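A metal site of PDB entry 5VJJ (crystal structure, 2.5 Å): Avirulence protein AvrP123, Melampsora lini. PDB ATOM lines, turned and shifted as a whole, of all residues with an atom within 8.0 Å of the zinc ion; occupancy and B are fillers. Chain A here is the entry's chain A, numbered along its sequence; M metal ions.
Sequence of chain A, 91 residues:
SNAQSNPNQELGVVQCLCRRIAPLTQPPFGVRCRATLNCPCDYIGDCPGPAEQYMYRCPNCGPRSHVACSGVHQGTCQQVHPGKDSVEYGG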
ATOM      1  N   VAL A  14      -5.373 -25.934 -23.792  1.00  0.00           N
ATOM      2  CA  VAL A  14      -6.082 -24.985 -22.931  1.00  0.00           C
ATOM      3  C   VAL A  14      -5.149 -23.822 -22.643  1.00  0.00           C
ATOM      4  O   VAL A  14      -3.924 -23.929 -22.717  1.00  0.00           O
ATOM      5  CB  VAL A  14      -6.555 -25.664 -21.621  1.00  0.00           C
ATOM      6  CG1 VAL A  14      -5.376 -26.052 -20.731  1.00  0.00           C
ATOM      7  CG2 VAL A  14      -7.527 -24.780 -20.872  1.00  0.00           C
ATOM      8  N   GLN A  15      -5.747 -22.682 -22.316  1.00  0.00           N
ATOM      9  CA  GLN A  15      -4.983 -21.527 -21.866  1.00  0.00           C
ATOM     10  C   GLN A  15      -4.695 -21.662 -20.372  1.00  0.00           C
ATOM     11  O   GLN A  15      -5.609 -21.789 -19.563  1.00  0.00           O
ATOM     12  CB  GLN A  15      -5.751 -20.238 -22.149  1.00  0.00           C
ATOM     13  CG  GLN A  15      -4.953 -18.978 -21.858  1.00  0.00           C
ATOM     14  CD  GLN A  15      -5.508 -17.743 -22.544  1.00  0.00           C
ATOM     15  OE1 GLN A  15      -6.724 -17.615 -22.732  1.00  0.00           O
ATOM     16  NE2 GLN A  15      -4.623 -16.837 -22.938  1.00  0.00           N
ATOM     17  N   CYS A  16      -3.409 -21.661 -20.016  1.00  0.00           N
ATOM     18  CA  CYS A  16      -3.016 -21.696 -18.619  1.00  0.00           C
ATOM     19  C   CYS A  16      -3.344 -20.360 -17.954  1.00  0.00           C
ATOM     20  O   CYS A  16      -3.611 -19.358 -18.616  1.00  0.00           O
ATOM     21  CB  CYS A  16      -1.513 -21.998 -18.500  1.00  0.00           C
ATOM     22  SG  CYS A  16      -0.827 -21.908 -16.812  1.00  0.00           S
ATOM     23  N   LEU A  17      -3.341 -20.365 -16.623  1.00  0.00           N
ATOM     24  CA  LEU A  17      -3.607 -19.125 -15.898  1.00  0.00           C
ATOM     25  C   LEU A  17      -2.580 -18.048 -16.217  1.00  0.00           C
ATOM     26  O   LEU A  17      -2.887 -16.861 -16.091  1.00  0.00           O
ATOM     27  CB  LEU A  17      -3.647 -19.398 -14.401  1.00  0.00           C
ATOM     28  CG  LEU A  17      -4.764 -20.332 -13.940  1.00  0.00           C
ATOM     29  CD1 LEU A  17      -4.584 -20.672 -12.466  1.00  0.00           C
ATOM     30  CD2 LEU A  17      -6.124 -19.702 -14.185  1.00  0.00           C
ATOM     31  N   CYS A  18      -1.373 -18.445 -16.600  1.00  0.00           N
ATOM     32  CA  CYS A  18      -0.386 -17.476 -17.075  1.00  0.00           C
ATOM     33  C   CYS A  18      -0.667 -17.001 -18.501  1.00  0.00           C
ATOM     34  O   CYS A  18       0.077 -16.159 -19.009  1.00  0.00           O
ATOM     35  CB  CYS A  18       1.018 -18.080 -16.999  1.00  0.00           C
ATOM     36  SG  CYS A  18       1.408 -19.237 -18.332  1.00  0.00           S
ATOM     37  N   ARG A  19      -1.710 -17.538 -19.135  1.00  0.00           N
ATOM     38  CA  ARG A  19      -2.254 -17.183 -20.440  1.00  0.00           C
ATOM     39  C   ARG A  19      -1.556 -17.904 -21.588  1.00  0.00           C
ATOM     40  O   ARG A  19      -2.003 -17.792 -22.729  1.00  0.00           O
ATOM     41  CB  ARG A  19      -2.244 -15.663 -20.710  1.00  0.00           C
ATOM     42  CG  ARG A  19      -3.188 -14.897 -19.812  1.00  0.00           C
ATOM     43  CD  ARG A  19      -3.354 -13.434 -20.216  1.00  0.00           C
ATOM     44  NE  ARG A  19      -2.210 -12.605 -19.821  1.00  0.00           N
ATOM     45  CZ  ARG A  19      -1.270 -12.148 -20.646  1.00  0.00           C
ATOM     46  NH1 ARG A  19      -1.316 -12.416 -21.951  1.00  0.00           N
ATOM     47  NH2 ARG A  19      -0.286 -11.402 -20.167  1.00  0.00           N
ATOM     48  N   ARG A  20      -0.484 -18.663 -21.337  1.00  0.00           N
ATOM     49  CA  ARG A  20       0.117 -19.469 -22.384  1.00  0.00           C
ATOM     50  C   ARG A  20      -0.792 -20.643 -22.735  1.00  0.00           C
ATOM     51  O   ARG A  20      -1.641 -21.064 -21.945  1.00  0.00           O
ATOM     52  CB  ARG A  20       1.489 -19.986 -21.960  1.00  0.00           C
ATOM     53  CG  ARG A  20       2.584 -18.938 -21.986  1.00  0.00           C
ATOM     54  CD  ARG A  20       3.838 -19.452 -21.322  1.00  0.00           C
ATOM     55  NE  ARG A  20       4.920 -18.460 -21.344  1.00  0.00           N
ATOM     56  CZ  ARG A  20       5.125 -17.555 -20.403  1.00  0.00           C
ATOM     57  NH1 ARG A  20       4.337 -17.494 -19.338  1.00  0.00           N
ATOM     58  NH2 ARG A  20       6.140 -16.705 -20.521  1.00  0.00           N
ATOM     59  N   ILE A  21      -0.592 -21.191 -23.927  1.00  0.00           N
ATOM     60  CA  ILE A  21      -1.351 -22.360 -24.360  1.00  0.00           C
ATOM     61  C   ILE A  21      -0.647 -23.607 -23.847  1.00  0.00           C
ATOM     62  O   ILE A  21       0.561 -23.790 -24.040  1.00  0.00           O
ATOM     63  CB  ILE A  21      -1.494 -22.381 -25.897  1.00  0.00           C
ATOM     64  CG1 ILE A  21      -2.141 -21.083 -26.393  1.00  0.00           C
ATOM     65  CG2 ILE A  21      -2.301 -23.587 -26.342  1.00  0.00           C
ATOM     66  CD1 ILE A  21      -3.518 -20.783 -25.798  1.00  0.00           C
ATOM     67  N   ALA A  22      -1.405 -24.471 -23.176  1.00  0.00           N
ATOM     68  CA  ALA A  22      -0.865 -25.672 -22.560  1.00  0.00           C
ATOM     69  C   ALA A  22      -1.606 -26.898 -23.057  1.00  0.00           C
ATOM     70  O   ALA A  22      -2.801 -26.827 -23.364  1.00  0.00           O
ATOM     71  CB  ALA A  22      -0.964 -25.602 -21.033  1.00  0.00           C
ATOM     72  N   TYR A  56      -3.188 -29.896 -17.114  1.00  0.00           N
ATOM     73  CA  TYR A  56      -2.319 -29.628 -18.245  1.00  0.00           C
ATOM     74  C   TYR A  56      -0.881 -29.477 -17.761  1.00  0.00           C
ATOM     75  O   TYR A  56      -0.605 -29.452 -16.556  1.00  0.00           O
ATOM     76  CB  TYR A  56      -2.775 -28.385 -19.008  1.00  0.00           C
ATOM     77  CG  TYR A  56      -3.086 -27.219 -18.103  1.00  0.00           C
ATOM     78  CD1 TYR A  56      -4.369 -26.996 -17.625  1.00  0.00           C
ATOM     79  CD2 TYR A  56      -2.084 -26.334 -17.720  1.00  0.00           C
ATOM     80  CE1 TYR A  56      -4.650 -25.925 -16.802  1.00  0.00           C
ATOM     81  CE2 TYR A  56      -2.356 -25.266 -16.907  1.00  0.00           C
ATOM     82  CZ  TYR A  56      -3.639 -25.060 -16.443  1.00  0.00           C
ATOM     83  OH  TYR A  56      -3.910 -23.988 -15.621  1.00  0.00           O
ATOM     84  N   ARG A  57       0.036 -29.390 -18.717  1.00  0.00           N
ATOM     85  CA  ARG A  57       1.464 -29.280 -18.477  1.00  0.00           C
ATOM     86  C   ARG A  57       1.949 -28.034 -19.217  1.00  0.00           C
ATOM     87  O   ARG A  57       2.274 -28.112 -20.398  1.00  0.00           O
ATOM     88  CB  ARG A  57       2.199 -30.539 -18.939  1.00  0.00           C
ATOM     89  CG  ARG A  57       3.711 -30.536 -18.704  1.00  0.00           C
ATOM     90  CD  ARG A  57       4.051 -31.020 -17.301  1.00  0.00           C
ATOM     91  NE  ARG A  57       3.920 -32.470 -17.172  1.00  0.00           N
ATOM     92  CZ  ARG A  57       4.934 -33.331 -17.266  1.00  0.00           C
ATOM     93  NH1 ARG A  57       6.175 -32.918 -17.473  1.00  0.00           N
ATOM     94  NH2 ARG A  57       4.692 -34.623 -17.131  1.00  0.00           N
ATOM     95  N   CYS A  58       1.988 -26.900 -18.517  1.00  0.00           N
ATOM     96  CA  CYS A  58       2.331 -25.645 -19.171  1.00  0.00           C
ATOM     97  C   CYS A  58       3.828 -25.605 -19.489  1.00  0.00           C
ATOM     98  O   CYS A  58       4.651 -25.935 -18.615  1.00  0.00           O
ATOM     99  CB  CYS A  58       1.974 -24.461 -18.281  1.00  0.00           C
ATOM    100  SG  CYS A  58       2.340 -22.859 -19.037  1.00  0.00           S
ATOM    101  N   PRO A  59       4.219 -25.199 -20.703  1.00  0.00           N
ATOM    102  CA  PRO A  59       5.663 -25.112 -20.993  1.00  0.00           C
ATOM    103  C   PRO A  59       6.401 -24.166 -20.064  1.00  0.00           C
ATOM    104  O   PRO A  59       7.605 -24.333 -19.857  1.00  0.00           O
ATOM    105  CB  PRO A  59       5.699 -24.598 -22.443  1.00  0.00           C
ATOM    106  CG  PRO A  59       4.401 -23.894 -22.617  1.00  0.00           C
ATOM    107  CD  PRO A  59       3.409 -24.689 -21.812  1.00  0.00           C
ATOM    108  N   ASN A  60       5.706 -23.187 -19.503  1.00  0.00           N
ATOM    109  CA  ASN A  60       6.300 -22.264 -18.539  1.00  0.00           C
ATOM    110  C   ASN A  60       6.139 -22.778 -17.110  1.00  0.00           C
ATOM    111  O   ASN A  60       7.133 -22.957 -16.396  1.00  0.00           O
ATOM    112  CB  ASN A  60       5.663 -20.883 -18.689  1.00  0.00           C
ATOM    113  CG  ASN A  60       6.242 -19.857 -17.736  1.00  0.00           C
ATOM    114  OD1 ASN A  60       7.357 -19.392 -17.922  1.00  0.00           O
ATOM    115  ND2 ASN A  60       5.472 -19.512 -16.711  1.00  0.00           N
ATOM    116  N   CYS A  61       4.905 -23.014 -16.696  1.00  0.00           N
ATOM    117  CA  CYS A  61       4.592 -23.341 -15.304  1.00  0.00           C
ATOM    118  C   CYS A  61       4.749 -24.814 -14.971  1.00  0.00           C
ATOM    119  O   CYS A  61       4.704 -25.168 -13.789  1.00  0.00           O
ATOM    120  CB  CYS A  61       3.159 -22.914 -14.980  1.00  0.00           C
ATOM    121  SG  CYS A  61       2.697 -21.302 -15.600  1.00  0.00           S
ATOM    122  N   GLY A  62       4.919 -25.689 -15.960  1.00  0.00           N
ATOM    123  CA  GLY A  62       4.905 -27.105 -15.702  1.00  0.00           C
ATOM    124  C   GLY A  62       3.531 -27.584 -15.278  1.00  0.00           C
ATOM    125  O   GLY A  62       2.525 -26.897 -15.492  1.00  0.00           O
ATOM    126  N   PRO A  63       3.459 -28.769 -14.657  1.00  0.00           N
ATOM    127  CA  PRO A  63       2.151 -29.311 -14.255  1.00  0.00           C
ATOM    128  C   PRO A  63       1.290 -28.323 -13.496  1.00  0.00           C
ATOM    129  O   PRO A  63       1.709 -27.795 -12.472  1.00  0.00           O
ATOM    130  CB  PRO A  63       2.538 -30.515 -13.370  1.00  0.00           C
ATOM    131  CG  PRO A  63       3.917 -30.913 -13.834  1.00  0.00           C
ATOM    132  CD  PRO A  63       4.584 -29.641 -14.284  1.00  0.00           C
ATOM    133  N   ARG A  64       0.075 -28.068 -13.982  1.00  0.00           N
ATOM    134  CA  ARG A  64      -0.808 -27.108 -13.330  1.00  0.00           C
ATOM    135  C   ARG A  64      -2.263 -27.471 -13.630  1.00  0.00           C
ATOM    136  O   ARG A  64      -2.552 -28.247 -14.544  1.00  0.00           O
ATOM    137  CB  ARG A  64      -0.510 -25.668 -13.788  1.00  0.00           C
ATOM    138  CG  ARG A  64      -1.175 -24.595 -12.942  1.00  0.00           C
ATOM    139  CD  ARG A  64      -0.692 -23.207 -13.294  1.00  0.00           C
ATOM    140  NE  ARG A  64      -1.194 -22.201 -12.367  1.00  0.00           N
ATOM    141  CZ  ARG A  64      -0.876 -20.906 -12.400  1.00  0.00           C
ATOM    142  NH1 ARG A  64      -0.031 -20.455 -13.325  1.00  0.00           N
ATOM    143  NH2 ARG A  64      -1.394 -20.066 -11.519  1.00  0.00           N
HETATM  144 ZN    ZN M   1       1.397 -21.405 -17.457  1.00  0.00          ZN
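NH1 of Arg 20 lies close to SG of Cys 18, at 3.6 Å. SG of Cys 61 lies close to ND2 of Asn 60, at 3.5 Å. N of Asn 60 sits close to SG of Cys 58 (3.4 Å). The side-chain sulfur of Cys 61 sits close to the guanidinium group of Arg 64 (3.7 Å).
Of the 18 residues printed, 4 come within 4 Å of the zinc ion. The nearest printed residue that does not touch the zinc ion is Asn 60 (4.5 Å).
The zinc ion is bound by SG of Cys 61 (2.3 Å), SG of Cys 18 (2.3 Å), SG of Cys 58 (2.3 Å) and SG of Cys 16 (2.4 Å).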
